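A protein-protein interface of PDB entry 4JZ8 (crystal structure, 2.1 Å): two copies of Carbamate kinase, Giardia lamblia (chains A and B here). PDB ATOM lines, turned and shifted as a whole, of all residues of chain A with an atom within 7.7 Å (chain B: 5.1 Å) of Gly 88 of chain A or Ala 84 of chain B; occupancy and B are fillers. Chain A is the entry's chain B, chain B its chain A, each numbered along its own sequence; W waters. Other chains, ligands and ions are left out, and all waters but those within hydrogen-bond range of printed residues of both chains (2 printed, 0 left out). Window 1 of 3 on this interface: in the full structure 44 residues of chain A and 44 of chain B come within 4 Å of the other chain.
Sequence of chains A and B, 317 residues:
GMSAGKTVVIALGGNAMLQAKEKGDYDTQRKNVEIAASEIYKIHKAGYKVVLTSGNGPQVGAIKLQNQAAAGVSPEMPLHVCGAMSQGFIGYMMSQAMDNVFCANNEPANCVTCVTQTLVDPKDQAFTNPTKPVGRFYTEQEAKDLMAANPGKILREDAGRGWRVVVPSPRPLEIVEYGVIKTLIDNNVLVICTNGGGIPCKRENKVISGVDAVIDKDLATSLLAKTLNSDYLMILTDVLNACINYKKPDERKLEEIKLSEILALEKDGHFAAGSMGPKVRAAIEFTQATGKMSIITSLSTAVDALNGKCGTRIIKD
O of Thr 113 of chain A sits at hydrogen-bond distance from N of Val 115 of chain B, at 3.0 Å.
N of Ile 199 of chain B lies close to NE2 of Gln 87 of chain B.
The backbone carbonyl oxygen (O) of Gly 91 of chain A is in hydrogen-bond range of the side-chain hydroxyl (OG1) of Thr 113 of chain A (2.7 Å).
The backbone carbonyl oxygen of Tyr 92 of chain A lies within hydrogen-bond range of the side-chain hydroxyl of Ser 95 of chain A.
Among the printed residues, pairs that only touch across the chains: Tyr 92 of chain A with His 80 of chain B, Ala 84 of chain A with Gly 88 of chain B, Gly 88 of chain A with Ala 84 of chain B, Phe 89 of chain A with Val 81 of chain B, Met 85 of chain A with Met 85 of chain B, Tyr 92 of chain A with Ile 199 of chain B, Tyr 92 of chain A with Ala 84 of chain B and Phe 89 of chain A with Met 85 of chain B.
Of the printed residues of chain B, Gly 88 of chain A touches Ala 84 (3.4 Å).
Of the printed residues of chain A, His 80 of chain B touches Tyr 92.
No residue of chain A comes within 4 Å of Gly 83 of chain B.
Ala 84 of chain B touches just these residues of chain A: Gly 88 and Tyr 92.
Of the printed residues of chain A, Met 85 of chain B touches Met 85 (3.5 Å) and Phe 89 (3.9 Å).
Gln 87 of chain B touches none of the printed residues of chain A.
Of the printed residues of chain A, Ile 199 of chain B touches Tyr 92 (3.7 Å).
The nearest residue of chain A that does not touch Ala 84 of chain B is Phe 89 of chain A (4.1 Å).
The nearest printed residue of chain B that does not touch Phe 89 of chain A is Ala 84 of chain B (4.1 Å).
Of the 11 printed residues of chain B, 7 touch a printed residue of chain A.
Printed residues of chain B that touch a printed residue of chain A: His 80, Val 81, Ala 84, Met 85, Gly 88, Val 115 and Ile 199.
Hydrophobic or aromatic side chains of chain B that line the printed part of chain A: His 80, Val 81, Ala 84, Met 85, Val 115 and Ile 199.
Printed residues of chain A that touch a printed residue of chain B: Ala 84, Met 85, Gly 88, Phe 89, Tyr 92 and Thr 113.
Hydrophobic or aromatic side chains of chain A within 4 Å of the printed part of chain B: Ala 84, Met 85, Phe 89 and Tyr 92.
Along chain A the printed residues that touch a printed residue of chain B span positions 84 to 113.
Ala 84 of chain A touches Gly 88 of chain B, and with the chains exchanged Gly 88 of chain A touches Ala 84 of chain B.
Met 85 of chain B touches its own counterpart, Met 85 of chain A.
Positions printed for both chains: 82, 83, 84, 85, 86, 87, 88, 115 and 199.
Of the 9 pairs that touch across the chains among the printed residues, 3 have their exchanged pair printed and touching as well.
Water W1 bridges O of Val 115 of chain B and N of Thr 113 of chain A.
Water W2 bridges the side-chain hydroxyl of Ser 95 of chain A (2.7 Å) and the backbone carbonyl oxygen of Val 115 of chain B (3.4 Å).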
ATOM      1  N   ILE A  63     -14.648 -10.572  21.237  1.00  0.00           N
ATOM      2  CA  ILE A  63     -14.453  -9.356  20.438  1.00  0.00           C
ATOM      3  C   ILE A  63     -13.573  -8.306  21.131  1.00  0.00           C
ATOM      4  O   ILE A  63     -12.635  -7.786  20.525  1.00  0.00           O
ATOM      5  CB  ILE A  63     -15.812  -8.724  19.984  1.00  0.00           C
ATOM      6  CG1 ILE A  63     -16.619  -9.728  19.144  1.00  0.00           C
ATOM      7  CG2 ILE A  63     -15.575  -7.445  19.152  1.00  0.00           C
ATOM      8  CD1 ILE A  63     -18.082  -9.272  18.766  1.00  0.00           C
ATOM      9  N   CYS A  82     -17.597  -2.838  20.434  1.00  0.00           N
ATOM     10  CA  CYS A  82     -17.601  -4.299  20.629  1.00  0.00           C
ATOM     11  C   CYS A  82     -19.006  -4.902  20.826  1.00  0.00           C
ATOM     12  O   CYS A  82     -19.311  -5.988  20.305  1.00  0.00           O
ATOM     13  CB  CYS A  82     -16.716  -4.700  21.819  1.00  0.00           C
ATOM     14  SG  CYS A  82     -14.998  -4.152  21.578  1.00  0.00           S
ATOM     15  N   GLY A  83     -19.835  -4.212  21.604  1.00  0.00           N
ATOM     16  CA  GLY A  83     -21.204  -4.671  21.870  1.00  0.00           C
ATOM     17  C   GLY A  83     -22.010  -4.674  20.580  1.00  0.00           C
ATOM     18  O   GLY A  83     -22.763  -5.618  20.310  1.00  0.00           O
ATOM     19  N   ALA A  84     -21.812  -3.612  19.786  1.00  0.00           N
ATOM     20  CA  ALA A  84     -22.475  -3.429  18.513  1.00  0.00           C
ATOM     21  C   ALA A  84     -22.083  -4.560  17.581  1.00  0.00           C
ATOM     22  O   ALA A  84     -22.897  -5.111  16.866  1.00  0.00           O
ATOM     23  CB  ALA A  84     -22.069  -2.114  17.909  1.00  0.00           C
ATOM     24  N   MET A  85     -20.806  -4.901  17.578  1.00  0.00           N
ATOM     25  CA  MET A  85     -20.328  -5.885  16.647  1.00  0.00           C
ATOM     26  C   MET A  85     -20.856  -7.248  17.019  1.00  0.00           C
ATOM     27  O   MET A  85     -21.131  -8.041  16.139  1.00  0.00           O
ATOM     28  CB  MET A  85     -18.797  -5.894  16.701  1.00  0.00           C
ATOM     29  CG  MET A  85     -18.190  -4.665  16.100  1.00  0.00           C
ATOM     30  SD  MET A  85     -16.349  -4.782  16.165  1.00  0.00           S
ATOM     31  CE  MET A  85     -15.886  -3.389  15.140  1.00  0.00           C
ATOM     32  N   SER A  86     -20.955  -7.542  18.327  1.00  0.00           N
ATOM     33  CA  SER A  86     -21.571  -8.786  18.788  1.00  0.00           C
ATOM     34  C   SER A  86     -23.045  -8.841  18.357  1.00  0.00           C
ATOM     35  O   SER A  86     -23.525  -9.903  18.010  1.00  0.00           O
ATOM     36  CB  SER A  86     -21.476  -8.969  20.321  1.00  0.00           C
ATOM     37  OG  SER A  86     -22.257  -7.989  21.022  1.00  0.00           O
ATOM     38  N   GLN A  87     -23.771  -7.725  18.392  1.00  0.00           N
ATOM     39  CA  GLN A  87     -25.184  -7.749  17.923  1.00  0.00           C
ATOM     40  C   GLN A  87     -25.232  -8.190  16.467  1.00  0.00           C
ATOM     41  O   GLN A  87     -26.036  -9.038  16.101  1.00  0.00           O
ATOM     42  CB  GLN A  87     -25.897  -6.374  18.067  1.00  0.00           C
ATOM     43  CG  GLN A  87     -26.062  -5.919  19.505  1.00  0.00           C
ATOM     44  CD  GLN A  87     -27.029  -4.798  19.666  1.00  0.00           C
ATOM     45  OE1 GLN A  87     -27.407  -4.133  18.683  1.00  0.00           O
ATOM     46  NE2 GLN A  87     -27.424  -4.535  20.911  1.00  0.00           N
ATOM     47  N   GLY A  88     -24.368  -7.605  15.627  1.00  0.00           N
ATOM     48  CA  GLY A  88     -24.307  -8.027  14.225  1.00  0.00           C
ATOM     49  C   GLY A  88     -24.120  -9.537  14.108  1.00  0.00           C
ATOM     50  O   GLY A  88     -24.769 -10.225  13.322  1.00  0.00           O
ATOM     51  N   PHE A  89     -23.205 -10.059  14.904  1.00  0.00           N
ATOM     52  CA  PHE A  89     -22.775 -11.445  14.736  1.00  0.00           C
ATOM     53  C   PHE A  89     -23.858 -12.326  15.337  1.00  0.00           C
ATOM     54  O   PHE A  89     -24.427 -13.196  14.667  1.00  0.00           O
ATOM     55  CB  PHE A  89     -21.391 -11.631  15.413  1.00  0.00           C
ATOM     56  CG  PHE A  89     -20.980 -13.068  15.625  1.00  0.00           C
ATOM     57  CD1 PHE A  89     -21.145 -14.023  14.620  1.00  0.00           C
ATOM     58  CD2 PHE A  89     -20.384 -13.453  16.821  1.00  0.00           C
ATOM     59  CE1 PHE A  89     -20.745 -15.340  14.828  1.00  0.00           C
ATOM     60  CE2 PHE A  89     -19.981 -14.760  17.022  1.00  0.00           C
ATOM     61  CZ  PHE A  89     -20.159 -15.709  16.023  1.00  0.00           C
ATOM     62  N   ILE A  90     -24.204 -12.065  16.586  1.00  0.00           N
ATOM     63  CA  ILE A  90     -25.253 -12.840  17.215  1.00  0.00           C
ATOM     64  C   ILE A  90     -26.591 -12.702  16.434  1.00  0.00           C
ATOM     65  O   ILE A  90     -27.301 -13.695  16.219  1.00  0.00           O
ATOM     66  CB  ILE A  90     -25.467 -12.416  18.684  1.00  0.00           C
ATOM     67  CG1 ILE A  90     -24.327 -12.892  19.588  1.00  0.00           C
ATOM     68  CG2 ILE A  90     -26.759 -13.019  19.203  1.00  0.00           C
ATOM     69  CD1 ILE A  90     -24.395 -12.267  21.042  1.00  0.00           C
ATOM     70  N   GLY A  91     -26.924 -11.482  16.007  1.00  0.00           N
ATOM     71  CA  GLY A  91     -28.160 -11.224  15.264  1.00  0.00           C
ATOM     72  C   GLY A  91     -28.184 -11.942  13.921  1.00  0.00           C
ATOM     73  O   GLY A  91     -29.243 -12.409  13.465  1.00  0.00           O
ATOM     74  N   TYR A  92     -27.013 -11.995  13.267  1.00  0.00           N
ATOM     75  CA  TYR A  92     -26.856 -12.733  12.026  1.00  0.00           C
ATOM     76  C   TYR A  92     -27.191 -14.207  12.250  1.00  0.00           C
ATOM     77  O   TYR A  92     -28.093 -14.765  11.583  1.00  0.00           O
ATOM     78  CB  TYR A  92     -25.416 -12.598  11.557  1.00  0.00           C
ATOM     79  CG  TYR A  92     -25.007 -13.539  10.461  1.00  0.00           C
ATOM     80  CD1 TYR A  92     -25.858 -13.826   9.398  1.00  0.00           C
ATOM     81  CD2 TYR A  92     -23.717 -14.105  10.454  1.00  0.00           C
ATOM     82  CE1 TYR A  92     -25.460 -14.690   8.356  1.00  0.00           C
ATOM     83  CE2 TYR A  92     -23.313 -14.959   9.422  1.00  0.00           C
ATOM     84  CZ  TYR A  92     -24.180 -15.240   8.376  1.00  0.00           C
ATOM     85  OH  TYR A  92     -23.757 -16.067   7.347  1.00  0.00           O
ATOM     86  N   MET A  93     -26.466 -14.854  13.184  1.00  0.00           N
ATOM     87  CA  MET A  93     -26.694 -16.284  13.464  1.00  0.00           C
ATOM     88  C   MET A  93     -28.174 -16.587  13.703  1.00  0.00           C
ATOM     89  O   MET A  93     -28.728 -17.543  13.141  1.00  0.00           O
ATOM     90  CB  MET A  93     -25.844 -16.782  14.649  1.00  0.00           C
ATOM     91  CG  MET A  93     -24.346 -16.904  14.316  1.00  0.00           C
ATOM     92  SD  MET A  93     -23.432 -17.881  15.536  1.00  0.00           S
ATOM     93  CE  MET A  93     -23.502 -16.721  16.938  1.00  0.00           C
ATOM     94  N   MET A  94     -28.824 -15.747  14.506  1.00  0.00           N
ATOM     95  CA  MET A  94     -30.199 -16.007  14.927  1.00  0.00           C
ATOM     96  C   MET A  94     -31.216 -15.768  13.803  1.00  0.00           C
ATOM     97  O   MET A  94     -32.115 -16.581  13.592  1.00  0.00           O
ATOM     98  CB  MET A  94     -30.549 -15.148  16.146  1.00  0.00           C
ATOM     99  CG  MET A  94     -29.741 -15.538  17.401  1.00  0.00           C
ATOM    100  SD  MET A  94     -30.330 -14.765  18.923  1.00  0.00           S
ATOM    101  CE  MET A  94     -29.304 -15.722  20.079  1.00  0.00           C
ATOM    102  N   SER A  95     -31.067 -14.659  13.092  1.00  0.00           N
ATOM    103  CA  SER A  95     -31.948 -14.348  11.946  1.00  0.00           C
ATOM    104  C   SER A  95     -31.878 -15.414  10.841  1.00  0.00           C
ATOM    105  O   SER A  95     -32.903 -15.832  10.259  1.00  0.00           O
ATOM    106  CB  SER A  95     -31.659 -12.944  11.386  1.00  0.00           C
ATOM    107  OG  SER A  95     -30.278 -12.787  11.123  1.00  0.00           O
ATOM    108  N   THR A 113     -33.193  -8.998  12.469  1.00  0.00           N
ATOM    109  CA  THR A 113     -32.473  -8.516  13.646  1.00  0.00           C
ATOM    110  C   THR A 113     -32.313  -7.000  13.615  1.00  0.00           C
ATOM    111  O   THR A 113     -31.820  -6.421  12.627  1.00  0.00           O
ATOM    112  CB  THR A 113     -31.063  -9.159  13.768  1.00  0.00           C
ATOM    113  OG1 THR A 113     -31.213 -10.591  13.792  1.00  0.00           O
ATOM    114  CG2 THR A 113     -30.364  -8.681  15.076  1.00  0.00           C
ATOM    115  N   CYS A 114     -32.724  -6.356  14.702  1.00  0.00           N
ATOM    116  CA  CYS A 114     -32.557  -4.911  14.845  1.00  0.00           C
ATOM    117  C   CYS A 114     -31.408  -4.570  15.781  1.00  0.00           C
ATOM    118  O   CYS A 114     -31.424  -4.973  16.931  1.00  0.00           O
ATOM    119  CB  CYS A 114     -33.823  -4.285  15.438  1.00  0.00           C
ATOM    120  SG  CYS A 114     -35.262  -4.342  14.353  1.00  0.00           S
ATOM    121  N   VAL A 115     -30.448  -3.789  15.299  1.00  0.00           N
ATOM    122  CA  VAL A 115     -29.388  -3.258  16.160  1.00  0.00           C
ATOM    123  C   VAL A 115     -30.057  -2.416  17.207  1.00  0.00           C
ATOM    124  O   VAL A 115     -31.062  -1.768  16.923  1.00  0.00           O
ATOM    125  CB  VAL A 115     -28.428  -2.361  15.340  1.00  0.00           C
ATOM    126  CG1 VAL A 115     -27.682  -1.355  16.253  1.00  0.00           C
ATOM    127  CG2 VAL A 115     -27.451  -3.213  14.501  1.00  0.00           C
ATOM    128  N   ASN A 195     -29.812  -7.770  21.586  1.00  0.00           N
ATOM    129  CA  ASN A 195     -28.838  -8.850  21.795  1.00  0.00           C
ATOM    130  C   ASN A 195     -27.762  -8.372  22.772  1.00  0.00           C
ATOM    131  O   ASN A 195     -27.116  -7.339  22.528  1.00  0.00           O
ATOM    132  CB  ASN A 195     -28.239  -9.314  20.444  1.00  0.00           C
ATOM    133  CG  ASN A 195     -29.301  -9.908  19.518  1.00  0.00           C
ATOM    134  OD1 ASN A 195     -29.759  -9.254  18.581  1.00  0.00           O
ATOM    135  ND2 ASN A 195     -29.756 -11.135  19.832  1.00  0.00           N
ATOM    136  N   ILE A 199     -26.821  -1.991  23.157  1.00  0.00           N
ATOM    137  CA  ILE A 199     -25.549  -1.259  23.208  1.00  0.00           C
ATOM    138  C   ILE A 199     -25.599  -0.145  24.249  1.00  0.00           C
ATOM    139  O   ILE A 199     -26.289   0.849  24.059  1.00  0.00           O
ATOM    140  CB  ILE A 199     -25.167  -0.642  21.823  1.00  0.00           C
ATOM    141  CG1 ILE A 199     -25.189  -1.731  20.747  1.00  0.00           C
ATOM    142  CG2 ILE A 199     -23.770   0.077  21.888  1.00  0.00           C
ATOM    143  CD1 ILE A 199     -25.538  -1.248  19.367  1.00  0.00           C
ATOM    144  N   HIS B  80     -17.501 -13.779   6.256  1.00  0.00           N
ATOM    145  CA  HIS B  80     -18.962 -13.457   6.257  1.00  0.00           C
ATOM    146  C   HIS B  80     -19.415 -13.080   7.638  1.00  0.00           C
ATOM    147  O   HIS B  80     -20.295 -12.217   7.773  1.00  0.00           O
ATOM    148  CB  HIS B  80     -19.860 -14.569   5.695  1.00  0.00           C
ATOM    149  CG  HIS B  80     -19.824 -15.849   6.471  1.00  0.00           C
ATOM    150  ND1 HIS B  80     -18.882 -16.837   6.245  1.00  0.00           N
ATOM    151  CD2 HIS B  80     -20.662 -16.351   7.417  1.00  0.00           C
ATOM    152  CE1 HIS B  80     -19.112 -17.864   7.041  1.00  0.00           C
ATOM    153  NE2 HIS B  80     -20.180 -17.583   7.780  1.00  0.00           N
ATOM    154  N   VAL B  81     -18.774 -13.688   8.658  1.00  0.00           N
ATOM    155  CA  VAL B  81     -19.061 -13.372  10.050  1.00  0.00           C
ATOM    156  C   VAL B  81     -18.477 -12.020  10.412  1.00  0.00           C
ATOM    157  O   VAL B  81     -19.047 -11.271  11.214  1.00  0.00           O
ATOM    158  CB  VAL B  81     -18.501 -14.461  11.060  1.00  0.00           C
ATOM    159  CG1 VAL B  81     -18.472 -13.912  12.466  1.00  0.00           C
ATOM    160  CG2 VAL B  81     -19.346 -15.705  11.044  1.00  0.00           C
ATOM    161  N   CYS B  82     -17.325 -11.705   9.834  1.00  0.00           N
ATOM    162  CA  CYS B  82     -16.747 -10.350   9.963  1.00  0.00           C
ATOM    163  C   CYS B  82     -17.667  -9.276   9.317  1.00  0.00           C
ATOM    164  O   CYS B  82     -17.775  -8.137   9.802  1.00  0.00           O
ATOM    165  CB  CYS B  82     -15.350 -10.304   9.340  1.00  0.00           C
ATOM    166  SG  CYS B  82     -14.062 -11.197  10.272  1.00  0.00           S
ATOM    167  N   GLY B  83     -18.302  -9.661   8.221  1.00  0.00           N
ATOM    168  CA  GLY B  83     -19.254  -8.799   7.514  1.00  0.00           C
ATOM    169  C   GLY B  83     -20.418  -8.473   8.426  1.00  0.00           C
ATOM    170  O   GLY B  83     -20.745  -7.304   8.619  1.00  0.00           O
ATOM    171  N   ALA B  84     -20.978  -9.503   9.070  1.00  0.00           N
ATOM    172  CA  ALA B  84     -22.016  -9.311  10.095  1.00  0.00           C
ATOM    173  C   ALA B  84     -21.613  -8.336  11.203  1.00  0.00           C
ATOM    174  O   ALA B  84     -22.373  -7.427  11.538  1.00  0.00           O
ATOM    175  CB  ALA B  84     -22.408 -10.633  10.698  1.00  0.00           C
ATOM    176  N   MET B  85     -20.431  -8.534  11.793  1.00  0.00           N
ATOM    177  CA  MET B  85     -19.950  -7.623  12.831  1.00  0.00           C
ATOM    178  C   MET B  85     -19.872  -6.163  12.360  1.00  0.00           C
ATOM    179  O   MET B  85     -20.202  -5.226  13.109  1.00  0.00           O
ATOM    180  CB  MET B  85     -18.556  -8.073  13.284  1.00  0.00           C
ATOM    181  CG  MET B  85     -18.557  -9.398  13.985  1.00  0.00           C
ATOM    182  SD  MET B  85     -16.930  -9.726  14.706  1.00  0.00           S
ATOM    183  CE  MET B  85     -17.210 -11.367  15.372  1.00  0.00           C
ATOM    184  N   SER B  86     -19.432  -5.977  11.116  1.00  0.00           N
ATOM    185  CA  SER B  86     -19.291  -4.639  10.519  1.00  0.00           C
ATOM    186  C   SER B  86     -20.648  -3.960  10.295  1.00  0.00           C
ATOM    187  O   SER B  86     -20.793  -2.752  10.471  1.00  0.00           O
ATOM    188  CB  SER B  86     -18.539  -4.712   9.212  1.00  0.00           C
ATOM    189  OG  SER B  86     -19.359  -5.243   8.180  1.00  0.00           O
ATOM    190  N   GLN B  87     -21.663  -4.732   9.933  1.00  0.00           N
ATOM    191  CA  GLN B  87     -23.022  -4.173   9.924  1.00  0.00           C
ATOM    192  C   GLN B  87     -23.404  -3.713  11.329  1.00  0.00           C
ATOM    193  O   GLN B  87     -23.982  -2.623  11.528  1.00  0.00           O
ATOM    194  CB  GLN B  87     -24.017  -5.225   9.435  1.00  0.00           C
ATOM    195  CG  GLN B  87     -23.790  -5.621   7.978  1.00  0.00           C
ATOM    196  CD  GLN B  87     -24.903  -6.441   7.475  1.00  0.00           C
ATOM    197  OE1 GLN B  87     -25.869  -6.617   8.196  1.00  0.00           O
ATOM    198  NE2 GLN B  87     -24.781  -7.003   6.262  1.00  0.00           N
ATOM    199  N   GLY B  88     -23.064  -4.533  12.311  1.00  0.00           N
ATOM    200  CA  GLY B  88     -23.308  -4.175  13.690  1.00  0.00           C
ATOM    201  C   GLY B  88     -22.673  -2.845  14.047  1.00  0.00           C
ATOM    202  O   GLY B  88     -23.321  -1.977  14.642  1.00  0.00           O
ATOM    203  N   VAL B 115     -29.843  -5.999  10.365  1.00  0.00           N
ATOM    204  CA  VAL B 115     -28.872  -6.963   9.864  1.00  0.00           C
ATOM    205  C   VAL B 115     -29.497  -7.553   8.601  1.00  0.00           C
ATOM    206  O   VAL B 115     -30.701  -7.900   8.583  1.00  0.00           O
ATOM    207  CB  VAL B 115     -28.586  -8.093  10.890  1.00  0.00           C
ATOM    208  CG1 VAL B 115     -27.561  -9.082  10.339  1.00  0.00           C
ATOM    209  CG2 VAL B 115     -28.137  -7.519  12.240  1.00  0.00           C
ATOM    210  N   ILE B 199     -24.590  -9.452   4.150  1.00  0.00           N
ATOM    211  CA  ILE B 199     -23.714 -10.582   4.488  1.00  0.00           C
ATOM    212  C   ILE B 199     -23.863 -11.588   3.352  1.00  0.00           C
ATOM    213  O   ILE B 199     -24.965 -12.044   3.054  1.00  0.00           O
ATOM    214  CB  ILE B 199     -24.123 -11.259   5.816  1.00  0.00           C
ATOM    215  CG1 ILE B 199     -23.909 -10.305   6.992  1.00  0.00           C
ATOM    216  CG2 ILE B 199     -23.279 -12.530   6.060  1.00  0.00           C
ATOM    217  CD1 ILE B 199     -25.026 -10.322   8.055  1.00  0.00           C
HETATM  218  O   HOH W   1     -31.800  -9.616   9.916  1.00  0.00           O
HETATM  219  O   HOH W   2     -30.092 -11.204   8.912  1.00  0.00           O
